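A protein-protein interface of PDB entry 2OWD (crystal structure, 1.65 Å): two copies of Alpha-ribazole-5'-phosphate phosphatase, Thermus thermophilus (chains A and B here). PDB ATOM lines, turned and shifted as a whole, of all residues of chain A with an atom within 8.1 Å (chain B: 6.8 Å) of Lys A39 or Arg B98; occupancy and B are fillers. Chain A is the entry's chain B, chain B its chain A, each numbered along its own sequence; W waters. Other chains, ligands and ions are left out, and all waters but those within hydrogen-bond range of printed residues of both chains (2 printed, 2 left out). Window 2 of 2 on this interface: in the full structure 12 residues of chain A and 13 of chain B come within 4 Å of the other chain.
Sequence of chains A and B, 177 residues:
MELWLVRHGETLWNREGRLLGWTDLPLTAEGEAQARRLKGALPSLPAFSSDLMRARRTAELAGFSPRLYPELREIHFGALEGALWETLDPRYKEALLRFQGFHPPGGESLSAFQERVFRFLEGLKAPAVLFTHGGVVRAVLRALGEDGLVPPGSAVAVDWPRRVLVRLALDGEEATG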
ATOM      1  N   ALA A  33       6.033 -42.418 -21.917  1.00  0.00           N
ATOM      2  CA  ALA A  33       7.363 -42.026 -21.463  1.00  0.00           C
ATOM      3  C   ALA A  33       7.886 -40.902 -22.361  1.00  0.00           C
ATOM      4  O   ALA A  33       8.519 -39.961 -21.885  1.00  0.00           O
ATOM      5  CB  ALA A  33       8.309 -43.220 -21.510  1.00  0.00           C
ATOM      6  N   GLN A  34       7.623 -41.008 -23.661  1.00  0.00           N
ATOM      7  CA  GLN A  34       8.060 -39.982 -24.601  1.00  0.00           C
ATOM      8  C   GLN A  34       7.369 -38.670 -24.250  1.00  0.00           C
ATOM      9  O   GLN A  34       7.979 -37.603 -24.291  1.00  0.00           O
ATOM     10  CB  GLN A  34       7.704 -40.377 -26.037  1.00  0.00           C
ATOM     11  CG  GLN A  34       8.652 -41.384 -26.658  1.00  0.00           C
ATOM     12  CD  GLN A  34       8.093 -42.011 -27.921  1.00  0.00           C
ATOM     13  OE1 GLN A  34       6.881 -42.048 -28.127  1.00  0.00           O
ATOM     14  NE2 GLN A  34       8.977 -42.518 -28.769  1.00  0.00           N
ATOM     15  N   ALA A  35       6.090 -38.757 -23.897  1.00  0.00           N
ATOM     16  CA  ALA A  35       5.321 -37.573 -23.538  1.00  0.00           C
ATOM     17  C   ALA A  35       5.891 -36.918 -22.282  1.00  0.00           C
ATOM     18  O   ALA A  35       6.032 -35.695 -22.223  1.00  0.00           O
ATOM     19  CB  ALA A  35       3.843 -37.941 -23.325  1.00  0.00           C
ATOM     20  N   ARG A  36       6.225 -37.725 -21.279  1.00  0.00           N
ATOM     21  CA  ARG A  36       6.778 -37.174 -20.044  1.00  0.00           C
ATOM     22  C   ARG A  36       8.096 -36.444 -20.292  1.00  0.00           C
ATOM     23  O   ARG A  36       8.381 -35.436 -19.651  1.00  0.00           O
ATOM     24  CB  ARG A  36       6.991 -38.275 -18.995  1.00  0.00           C
ATOM     25  CG  ARG A  36       5.709 -38.938 -18.519  1.00  0.00           C
ATOM     26  CD  ARG A  36       5.941 -39.720 -17.228  1.00  0.00           C
ATOM     27  NE  ARG A  36       4.769 -40.507 -16.853  1.00  0.00           N
ATOM     28  CZ  ARG A  36       4.462 -41.689 -17.382  1.00  0.00           C
ATOM     29  NH1 ARG A  36       5.243 -42.232 -18.307  1.00  0.00           N
ATOM     30  NH2 ARG A  36       3.362 -42.322 -16.998  1.00  0.00           N
ATOM     31  N   ARG A  37       8.899 -36.948 -21.222  1.00  0.00           N
ATOM     32  CA  ARG A  37      10.179 -36.318 -21.522  1.00  0.00           C
ATOM     33  C   ARG A  37      10.034 -34.923 -22.123  1.00  0.00           C
ATOM     34  O   ARG A  37      10.960 -34.116 -22.055  1.00  0.00           O
ATOM     35  CB  ARG A  37      11.010 -37.202 -22.456  1.00  0.00           C
ATOM     36  CG  ARG A  37      11.680 -38.376 -21.753  1.00  0.00           C
ATOM     37  CD  ARG A  37      12.765 -38.997 -22.623  1.00  0.00           C
ATOM     38  NE  ARG A  37      12.225 -39.901 -23.632  1.00  0.00           N
ATOM     39  CZ  ARG A  37      11.738 -41.110 -23.367  1.00  0.00           C
ATOM     40  NH1 ARG A  37      11.723 -41.564 -22.120  1.00  0.00           N
ATOM     41  NH2 ARG A  37      11.270 -41.868 -24.349  1.00  0.00           N
ATOM     42  N   LEU A  38       8.872 -34.637 -22.704  1.00  0.00           N
ATOM     43  CA  LEU A  38       8.623 -33.330 -23.305  1.00  0.00           C
ATOM     44  C   LEU A  38       8.361 -32.244 -22.260  1.00  0.00           C
ATOM     45  O   LEU A  38       8.511 -31.054 -22.545  1.00  0.00           O
ATOM     46  CB  LEU A  38       7.434 -33.414 -24.266  1.00  0.00           C
ATOM     47  CG  LEU A  38       7.698 -34.172 -25.571  1.00  0.00           C
ATOM     48  CD1 LEU A  38       6.385 -34.435 -26.305  1.00  0.00           C
ATOM     49  CD2 LEU A  38       8.645 -33.354 -26.436  1.00  0.00           C
ATOM     50  N   LYS A  39       7.974 -32.652 -21.053  1.00  0.00           N
ATOM     51  CA  LYS A  39       7.688 -31.690 -19.991  1.00  0.00           C
ATOM     52  C   LYS A  39       8.874 -30.770 -19.698  1.00  0.00           C
ATOM     53  O   LYS A  39       8.697 -29.583 -19.437  1.00  0.00           O
ATOM     54  CB  LYS A  39       7.272 -32.411 -18.703  1.00  0.00           C
ATOM     55  CG  LYS A  39       6.772 -31.458 -17.616  1.00  0.00           C
ATOM     56  CD  LYS A  39       6.151 -32.196 -16.430  1.00  0.00           C
ATOM     57  CE  LYS A  39       5.652 -31.211 -15.381  1.00  0.00           C
ATOM     58  NZ  LYS A  39       5.047 -31.882 -14.194  1.00  0.00           N
ATOM     59  N   GLY A  40      10.084 -31.313 -19.749  1.00  0.00           N
ATOM     60  CA  GLY A  40      11.251 -30.493 -19.470  1.00  0.00           C
ATOM     61  C   GLY A  40      11.843 -29.799 -20.682  1.00  0.00           C
ATOM     62  O   GLY A  40      12.993 -29.350 -20.643  1.00  0.00           O
ATOM     63  N   ALA A  41      11.065 -29.686 -21.754  1.00  0.00           N
ATOM     64  CA  ALA A  41      11.559 -29.060 -22.973  1.00  0.00           C
ATOM     65  C   ALA A  41      10.635 -28.009 -23.574  1.00  0.00           C
ATOM     66  O   ALA A  41      11.077 -26.921 -23.934  1.00  0.00           O
ATOM     67  CB  ALA A  41      11.846 -30.131 -24.013  1.00  0.00           C
ATOM     68  N   LEU A  42       9.352 -28.333 -23.684  1.00  0.00           N
ATOM     69  CA  LEU A  42       8.385 -27.418 -24.293  1.00  0.00           C
ATOM     70  C   LEU A  42       8.147 -26.130 -23.511  1.00  0.00           C
ATOM     71  O   LEU A  42       8.023 -26.152 -22.287  1.00  0.00           O
ATOM     72  CB  LEU A  42       7.053 -28.145 -24.499  1.00  0.00           C
ATOM     73  CG  LEU A  42       7.114 -29.371 -25.416  1.00  0.00           C
ATOM     74  CD1 LEU A  42       5.774 -30.091 -25.408  1.00  0.00           C
ATOM     75  CD2 LEU A  42       7.481 -28.931 -26.829  1.00  0.00           C
ATOM     76  N   PRO A  43       8.076 -24.985 -24.217  1.00  0.00           N
ATOM     77  CA  PRO A  43       7.844 -23.692 -23.565  1.00  0.00           C
ATOM     78  C   PRO A  43       6.405 -23.620 -23.058  1.00  0.00           C
ATOM     79  O   PRO A  43       5.521 -24.273 -23.605  1.00  0.00           O
ATOM     80  CB  PRO A  43       8.114 -22.690 -24.682  1.00  0.00           C
ATOM     81  CG  PRO A  43       7.620 -23.424 -25.903  1.00  0.00           C
ATOM     82  CD  PRO A  43       8.183 -24.826 -25.680  1.00  0.00           C
ATOM     83  N   SER A  44       6.173 -22.822 -22.021  1.00  0.00           N
ATOM     84  CA  SER A  44       4.836 -22.700 -21.456  1.00  0.00           C
ATOM     85  C   SER A  44       3.956 -21.698 -22.203  1.00  0.00           C
ATOM     86  O   SER A  44       3.528 -20.682 -21.646  1.00  0.00           O
ATOM     87  CB  SER A  44       4.934 -22.334 -19.974  1.00  0.00           C
ATOM     88  OG  SER A  44       5.895 -21.313 -19.770  1.00  0.00           O
ATOM     89  N   LEU A  45       3.688 -21.998 -23.471  1.00  0.00           N
ATOM     90  CA  LEU A  45       2.844 -21.153 -24.316  1.00  0.00           C
ATOM     91  C   LEU A  45       1.432 -21.717 -24.263  1.00  0.00           C
ATOM     92  O   LEU A  45       1.232 -22.833 -23.790  1.00  0.00           O
ATOM     93  CB  LEU A  45       3.318 -21.199 -25.764  1.00  0.00           C
ATOM     94  CG  LEU A  45       4.804 -21.009 -26.055  1.00  0.00           C
ATOM     95  CD1 LEU A  45       5.005 -20.961 -27.557  1.00  0.00           C
ATOM     96  CD2 LEU A  45       5.307 -19.722 -25.404  1.00  0.00           C
ATOM     97  N   THR A  58      -0.771 -37.021 -24.414  1.00  0.00           N
ATOM     98  CA  THR A  58       0.583 -36.516 -24.593  1.00  0.00           C
ATOM     99  C   THR A  58       0.670 -35.120 -23.972  1.00  0.00           C
ATOM    100  O   THR A  58       1.618 -34.808 -23.257  1.00  0.00           O
ATOM    101  CB  THR A  58       0.962 -36.432 -26.081  1.00  0.00           C
ATOM    102  OG1 THR A  58       0.971 -37.749 -26.644  1.00  0.00           O
ATOM    103  CG2 THR A  58       2.342 -35.814 -26.245  1.00  0.00           C
ATOM    104  N   ALA A  59      -0.337 -34.292 -24.237  1.00  0.00           N
ATOM    105  CA  ALA A  59      -0.372 -32.936 -23.696  1.00  0.00           C
ATOM    106  C   ALA A  59      -0.371 -32.959 -22.171  1.00  0.00           C
ATOM    107  O   ALA A  59       0.338 -32.186 -21.528  1.00  0.00           O
ATOM    108  CB  ALA A  59      -1.609 -32.206 -24.203  1.00  0.00           C
ATOM    109  N   GLU A  60      -1.182 -33.842 -21.599  1.00  0.00           N
ATOM    110  CA  GLU A  60      -1.294 -33.978 -20.142  1.00  0.00           C
ATOM    111  C   GLU A  60       0.045 -34.350 -19.502  1.00  0.00           C
ATOM    112  O   GLU A  60       0.507 -33.736 -18.543  1.00  0.00           O
ATOM    113  CB  GLU A  60      -2.362 -35.035 -19.805  1.00  0.00           C
ATOM    114  CG  GLU A  60      -2.324 -35.482 -18.339  1.00  0.00           C
ATOM    115  CD  GLU A  60      -3.425 -36.486 -18.049  1.00  0.00           C
ATOM    116  OE1 GLU A  60      -3.633 -37.384 -18.849  1.00  0.00           O
ATOM    117  OE2 GLU A  60      -4.042 -36.388 -16.984  1.00  0.00           O
ATOM    118  N   LEU A  61       0.673 -35.412 -20.044  1.00  0.00           N
ATOM    119  CA  LEU A  61       1.942 -35.879 -19.489  1.00  0.00           C
ATOM    120  C   LEU A  61       3.081 -34.874 -19.716  1.00  0.00           C
ATOM    121  O   LEU A  61       4.097 -34.878 -19.036  1.00  0.00           O
ATOM    122  CB  LEU A  61       2.296 -37.214 -20.145  1.00  0.00           C
ATOM    123  CG  LEU A  61       1.422 -38.366 -19.645  1.00  0.00           C
ATOM    124  CD1 LEU A  61       1.795 -39.700 -20.296  1.00  0.00           C
ATOM    125  CD2 LEU A  61       1.528 -38.582 -18.136  1.00  0.00           C
ATOM    126  N   ALA A  62       2.898 -34.024 -20.745  1.00  0.00           N
ATOM    127  CA  ALA A  62       3.898 -32.989 -21.000  1.00  0.00           C
ATOM    128  C   ALA A  62       3.703 -31.770 -20.090  1.00  0.00           C
ATOM    129  O   ALA A  62       4.455 -30.806 -20.124  1.00  0.00           O
ATOM    130  CB  ALA A  62       3.799 -32.572 -22.470  1.00  0.00           C
ATOM    131  N   GLY A  63       2.618 -31.814 -19.288  1.00  0.00           N
ATOM    132  CA  GLY A  63       2.406 -30.754 -18.301  1.00  0.00           C
ATOM    133  C   GLY A  63       1.479 -29.645 -18.817  1.00  0.00           C
ATOM    134  O   GLY A  63       1.504 -28.514 -18.350  1.00  0.00           O
ATOM    135  N   PHE A  64       0.621 -29.950 -19.788  1.00  0.00           N
ATOM    136  CA  PHE A  64      -0.290 -28.953 -20.360  1.00  0.00           C
ATOM    137  C   PHE A  64      -1.776 -29.315 -20.165  1.00  0.00           C
ATOM    138  O   PHE A  64      -2.150 -30.473 -19.912  1.00  0.00           O
ATOM    139  CB  PHE A  64      -0.013 -28.819 -21.868  1.00  0.00           C
ATOM    140  CG  PHE A  64       1.341 -28.214 -22.141  1.00  0.00           C
ATOM    141  CD1 PHE A  64       2.459 -29.037 -22.226  1.00  0.00           C
ATOM    142  CD2 PHE A  64       1.462 -26.852 -22.389  1.00  0.00           C
ATOM    143  CE1 PHE A  64       3.701 -28.492 -22.531  1.00  0.00           C
ATOM    144  CE2 PHE A  64       2.713 -26.315 -22.696  1.00  0.00           C
ATOM    145  CZ  PHE A  64       3.835 -27.131 -22.764  1.00  0.00           C
ATOM    146  N   SER A  65      -2.606 -28.245 -20.267  1.00  0.00           N
ATOM    147  CA  SER A  65      -4.069 -28.343 -20.252  1.00  0.00           C
ATOM    148  C   SER A  65      -4.635 -27.607 -21.485  1.00  0.00           C
ATOM    149  O   SER A  65      -5.015 -26.441 -21.449  1.00  0.00           O
ATOM    150  CB  SER A  65      -4.559 -27.647 -18.980  1.00  0.00           C
ATOM    151  OG  SER A  65      -4.047 -28.343 -17.844  1.00  0.00           O
ATOM    152  N   PHE A 131      -0.446 -29.942 -29.827  1.00  0.00           N
ATOM    153  CA  PHE A 131      -0.276 -31.385 -29.702  1.00  0.00           C
ATOM    154  C   PHE A 131      -1.121 -31.977 -30.811  1.00  0.00           C
ATOM    155  O   PHE A 131      -2.352 -31.911 -30.786  1.00  0.00           O
ATOM    156  CB  PHE A 131      -0.728 -31.833 -28.313  1.00  0.00           C
ATOM    157  CG  PHE A 131       0.208 -31.391 -27.232  1.00  0.00           C
ATOM    158  CD1 PHE A 131       1.337 -32.148 -26.917  1.00  0.00           C
ATOM    159  CD2 PHE A 131       0.010 -30.179 -26.581  1.00  0.00           C
ATOM    160  CE1 PHE A 131       2.256 -31.697 -25.966  1.00  0.00           C
ATOM    161  CE2 PHE A 131       0.929 -29.717 -25.626  1.00  0.00           C
ATOM    162  CZ  PHE A 131       2.049 -30.477 -25.321  1.00  0.00           C
ATOM    163  N   LEU A 168      13.273 -30.672 -32.163  1.00  0.00           N
ATOM    164  CA  LEU A 168      13.546 -31.317 -30.890  1.00  0.00           C
ATOM    165  C   LEU A 168      13.225 -32.801 -30.994  1.00  0.00           C
ATOM    166  O   LEU A 168      12.086 -33.220 -30.784  1.00  0.00           O
ATOM    167  CB  LEU A 168      12.696 -30.685 -29.786  1.00  0.00           C
ATOM    168  CG  LEU A 168      12.939 -31.204 -28.368  1.00  0.00           C
ATOM    169  CD1 LEU A 168      14.294 -30.708 -27.874  1.00  0.00           C
ATOM    170  CD2 LEU A 168      11.831 -30.729 -27.444  1.00  0.00           C
ATOM    171  N   LEU A 170      13.923 -36.292 -29.385  1.00  0.00           N
ATOM    172  CA  LEU A 170      14.439 -36.947 -28.192  1.00  0.00           C
ATOM    173  C   LEU A 170      14.451 -38.466 -28.339  1.00  0.00           C
ATOM    174  O   LEU A 170      14.126 -38.957 -29.442  1.00  0.00           O
ATOM    175  CB  LEU A 170      13.597 -36.549 -26.977  1.00  0.00           C
ATOM    176  CG  LEU A 170      13.485 -35.050 -26.685  1.00  0.00           C
ATOM    177  CD1 LEU A 170      12.577 -34.837 -25.483  1.00  0.00           C
ATOM    178  CD2 LEU A 170      14.865 -34.463 -26.422  1.00  0.00           C
ATOM    179  N   LYS B  93      -4.160 -22.749  -6.892  1.00  0.00           N
ATOM    180  CA  LYS B  93      -2.833 -22.152  -6.824  1.00  0.00           C
ATOM    181  C   LYS B  93      -1.953 -22.599  -7.992  1.00  0.00           C
ATOM    182  O   LYS B  93      -1.335 -21.798  -8.680  1.00  0.00           O
ATOM    183  CB  LYS B  93      -2.187 -22.557  -5.498  1.00  0.00           C
ATOM    184  CG  LYS B  93      -2.156 -21.405  -4.491  1.00  0.00           C
ATOM    185  CD  LYS B  93      -1.002 -21.541  -3.495  1.00  0.00           C
ATOM    186  CE  LYS B  93      -1.059 -20.489  -2.383  1.00  0.00           C
ATOM    187  NZ  LYS B  93      -1.764 -21.033  -1.224  1.00  0.00           N
ATOM    188  N   GLU B  94      -1.873 -23.930  -8.187  1.00  0.00           N
ATOM    189  CA  GLU B  94      -1.026 -24.431  -9.264  1.00  0.00           C
ATOM    190  C   GLU B  94      -1.585 -24.085 -10.645  1.00  0.00           C
ATOM    191  O   GLU B  94      -0.859 -23.857 -11.601  1.00  0.00           O
ATOM    192  CB  GLU B  94      -0.869 -25.944  -9.131  1.00  0.00           C
ATOM    193  CG  GLU B  94      -0.547 -26.600 -10.477  1.00  0.00           C
ATOM    194  CD  GLU B  94       0.071 -27.959 -10.249  1.00  0.00           C
ATOM    195  OE1 GLU B  94      -0.616 -28.837  -9.747  1.00  0.00           O
ATOM    196  OE2 GLU B  94       1.234 -28.140 -10.607  1.00  0.00           O
ATOM    197  N   ALA B  95      -2.926 -24.097 -10.752  1.00  0.00           N
ATOM    198  CA  ALA B  95      -3.521 -23.690 -12.016  1.00  0.00           C
ATOM    199  C   ALA B  95      -3.033 -22.294 -12.403  1.00  0.00           C
ATOM    200  O   ALA B  95      -2.661 -22.018 -13.536  1.00  0.00           O
ATOM    201  CB  ALA B  95      -5.041 -23.681 -11.854  1.00  0.00           C
ATOM    202  N   LEU B  96      -3.073 -21.390 -11.411  1.00  0.00           N
ATOM    203  CA  LEU B  96      -2.631 -20.026 -11.661  1.00  0.00           C
ATOM    204  C   LEU B  96      -1.106 -19.938 -11.845  1.00  0.00           C
ATOM    205  O   LEU B  96      -0.591 -19.157 -12.638  1.00  0.00           O
ATOM    206  CB  LEU B  96      -3.088 -19.158 -10.486  1.00  0.00           C
ATOM    207  CG  LEU B  96      -4.607 -18.950 -10.466  1.00  0.00           C
ATOM    208  CD1 LEU B  96      -5.076 -18.133  -9.258  1.00  0.00           C
ATOM    209  CD2 LEU B  96      -5.118 -18.212 -11.703  1.00  0.00           C
ATOM    210  N   LEU B  97      -0.380 -20.749 -11.052  1.00  0.00           N
ATOM    211  CA  LEU B  97       1.072 -20.745 -11.168  1.00  0.00           C
ATOM    212  C   LEU B  97       1.515 -21.220 -12.556  1.00  0.00           C
ATOM    213  O   LEU B  97       2.367 -20.621 -13.211  1.00  0.00           O
ATOM    214  CB  LEU B  97       1.642 -21.674 -10.089  1.00  0.00           C
ATOM    215  CG  LEU B  97       1.533 -21.087  -8.677  1.00  0.00           C
ATOM    216  CD1 LEU B  97       2.079 -22.038  -7.610  1.00  0.00           C
ATOM    217  CD2 LEU B  97       2.305 -19.778  -8.514  1.00  0.00           C
ATOM    218  N   ARG B  98       0.933 -22.360 -12.987  1.00  0.00           N
ATOM    219  CA  ARG B  98       1.307 -22.905 -14.286  1.00  0.00           C
ATOM    220  C   ARG B  98       0.551 -22.211 -15.435  1.00  0.00           C
ATOM    221  O   ARG B  98       0.770 -22.481 -16.612  1.00  0.00           O
ATOM    222  CB  ARG B  98       0.995 -24.406 -14.291  1.00  0.00           C
ATOM    223  CG  ARG B  98       1.778 -25.164 -13.215  1.00  0.00           C
ATOM    224  CD  ARG B  98       1.526 -26.680 -13.245  1.00  0.00           C
ATOM    225  NE  ARG B  98       1.910 -27.270 -14.540  1.00  0.00           N
ATOM    226  CZ  ARG B  98       3.227 -27.375 -14.854  1.00  0.00           C
ATOM    227  NH1 ARG B  98       4.180 -26.926 -14.035  1.00  0.00           N
ATOM    228  NH2 ARG B  98       3.574 -27.945 -16.013  1.00  0.00           N
ATOM    229  N   PHE B  99      -0.399 -21.326 -15.036  1.00  0.00           N
ATOM    230  CA  PHE B  99      -1.204 -20.557 -15.998  1.00  0.00           C
ATOM    231  C   PHE B  99      -1.972 -21.466 -16.964  1.00  0.00           C
ATOM    232  O   PHE B  99      -1.935 -21.273 -18.170  1.00  0.00           O
ATOM    233  CB  PHE B  99      -0.298 -19.595 -16.783  1.00  0.00           C
ATOM    234  CG  PHE B  99      -1.021 -18.300 -17.094  1.00  0.00           C
ATOM    235  CD1 PHE B  99      -1.362 -17.433 -16.060  1.00  0.00           C
ATOM    236  CD2 PHE B  99      -1.283 -17.943 -18.410  1.00  0.00           C
ATOM    237  CE1 PHE B  99      -1.978 -16.212 -16.347  1.00  0.00           C
ATOM    238  CE2 PHE B  99      -1.901 -16.718 -18.689  1.00  0.00           C
ATOM    239  CZ  PHE B  99      -2.250 -15.858 -17.661  1.00  0.00           C
ATOM    240  N   GLN B 100      -2.694 -22.446 -16.431  1.00  0.00           N
ATOM    241  CA  GLN B 100      -3.472 -23.345 -17.274  1.00  0.00           C
ATOM    242  C   GLN B 100      -4.508 -24.113 -16.470  1.00  0.00           C
ATOM    243  O   GLN B 100      -4.344 -24.317 -15.265  1.00  0.00           O
ATOM    244  CB  GLN B 100      -2.543 -24.338 -17.960  1.00  0.00           C
ATOM    245  CG  GLN B 100      -1.912 -25.319 -16.996  1.00  0.00           C
ATOM    246  CD  GLN B 100      -0.887 -26.207 -17.658  1.00  0.00           C
ATOM    247  OE1 GLN B 100      -0.430 -25.925 -18.767  1.00  0.00           O
ATOM    248  NE2 GLN B 100      -0.525 -27.291 -16.989  1.00  0.00           N
ATOM    249  N   GLY B 101      -5.574 -24.530 -17.146  1.00  0.00           N
ATOM    250  CA  GLY B 101      -6.621 -25.294 -16.496  1.00  0.00           C
ATOM    251  C   GLY B 101      -7.205 -24.647 -15.255  1.00  0.00           C
ATOM    252  O   GLY B 101      -7.273 -25.267 -14.189  1.00  0.00           O
ATOM    253  N   LEU B 110      -9.149 -19.593 -17.749  1.00  0.00           N
ATOM    254  CA  LEU B 110      -7.937 -18.976 -18.267  1.00  0.00           C
ATOM    255  C   LEU B 110      -7.916 -19.012 -19.794  1.00  0.00           C
ATOM    256  O   LEU B 110      -7.411 -18.092 -20.431  1.00  0.00           O
ATOM    257  CB  LEU B 110      -6.695 -19.664 -17.699  1.00  0.00           C
ATOM    258  CG  LEU B 110      -6.051 -18.945 -16.509  1.00  0.00           C
ATOM    259  CD1 LEU B 110      -4.865 -19.746 -15.992  1.00  0.00           C
ATOM    260  CD2 LEU B 110      -5.593 -17.554 -16.949  1.00  0.00           C
ATOM    261  N   ARG B 138       0.682 -10.688 -17.844  1.00  0.00           N
ATOM    262  CA  ARG B 138       1.229 -12.025 -17.683  1.00  0.00           C
ATOM    263  C   ARG B 138       0.873 -12.924 -18.864  1.00  0.00           C
ATOM    264  O   ARG B 138       1.714 -13.671 -19.350  1.00  0.00           O
ATOM    265  CB  ARG B 138       0.734 -12.656 -16.377  1.00  0.00           C
ATOM    266  CG  ARG B 138       1.480 -13.932 -16.031  1.00  0.00           C
ATOM    267  CD  ARG B 138       1.053 -14.505 -14.693  1.00  0.00           C
ATOM    268  NE  ARG B 138       1.686 -15.802 -14.482  1.00  0.00           N
ATOM    269  CZ  ARG B 138       1.196 -16.755 -13.697  1.00  0.00           C
ATOM    270  NH1 ARG B 138       0.062 -16.559 -13.037  1.00  0.00           N
ATOM    271  NH2 ARG B 138       1.825 -17.915 -13.600  1.00  0.00           N
ATOM    272  N   ARG B 142       3.869 -14.472 -21.022  1.00  0.00           N
ATOM    273  CA  ARG B 142       4.003 -15.925 -21.095  1.00  0.00           C
ATOM    274  C   ARG B 142       3.885 -16.445 -22.529  1.00  0.00           C
ATOM    275  O   ARG B 142       4.558 -17.408 -22.902  1.00  0.00           O
ATOM    276  CB  ARG B 142       2.963 -16.613 -20.204  1.00  0.00           C
ATOM    277  CG  ARG B 142       3.328 -16.624 -18.727  1.00  0.00           C
ATOM    278  CD  ARG B 142       2.320 -17.436 -17.906  1.00  0.00           C
ATOM    279  NE  ARG B 142       2.615 -18.871 -17.896  1.00  0.00           N
ATOM    280  CZ  ARG B 142       3.526 -19.440 -17.108  1.00  0.00           C
ATOM    281  NH1 ARG B 142       4.233 -18.705 -16.264  1.00  0.00           N
ATOM    282  NH2 ARG B 142       3.733 -20.744 -17.166  1.00  0.00           N
HETATM  283  O   HOH W   1       6.110 -19.059 -21.222  1.00  0.00           O
HETATM  284  O   HOH W   2       1.914 -21.202 -19.031  1.00  0.00           O
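The guanidinium group of Arg B98 is in hydrogen-bond range of the backbone carbonyl oxygen of Gly A63 (3.2 Å).
NE2 of Gln B100 sits at hydrogen-bond distance from O of Gly A63, 2.7 Å away.
OG of Ser A44 lies within hydrogen-bond range of NH2 of Arg B142 (3.4 Å).
The backbone NH (N) of Phe A64 sits at hydrogen-bond distance from the backbone carbonyl oxygen (O) of Ala A59.
The side-chain amide nitrogen of Gln B100 lies close to the guanidinium group of Arg B98, at 3.5 Å.
NH2 of Arg B142 lies within hydrogen-bond range of O of Arg B98, 3.5 Å away.
The backbone carbonyl oxygen (O) of Ala B95 lies within hydrogen-bond range of the backbone NH (N) of Gln B100.
CE of Lys A39 touches NH2 of Arg B98, 3.9 Å away.
Leu A45 touches Arg B142 (CD2 to O, 3.5 Å).
Gln B100 touches Phe A64.
N of Ser A65 touches OE1 of Gln B100, 3.5 Å away.
Ser A65 touches Gly B101.
Lys A39 touches one residue of chain B.
Arg B98 touches just these residues of chain A: Lys A39 (3.9 Å) and Gly A63 (3.2 Å).
Of the printed residues of chain B, Gly A63 touches Arg B98 and Gln B100.
Of the printed residues of chain B, Leu A45 touches Arg B142.
Of the printed residues of chain B, Ser A65 touches Gln B100 and Gly B101.
The nearest residue of chain A that does not touch Arg B98 is Ala A62 (5.1 Å).
The nearest printed residue of chain B that does not touch Ser A44 is Arg B98 (5.4 Å).
Printed residues of chain B that touch a printed residue of chain A: Arg B98, Gln B100, Gly B101 and Arg B142.
Among the printed residues, 8 pairs touch across the chains.
No position is printed for both chains.
Of the 8 pairs that touch across the chains among the printed residues, none has its exchanged pair printed and touching as well.
Water W2 lies within hydrogen-bond range of the guanidinium group of Arg B142, the backbone carbonyl oxygen of Arg B98 and the backbone carbonyl oxygen of Ser A44.
Water W1 lies within hydrogen-bond range of the side-chain hydroxyl (OG) of Ser A44 and the backbone carbonyl oxygen (O) of Arg B142.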
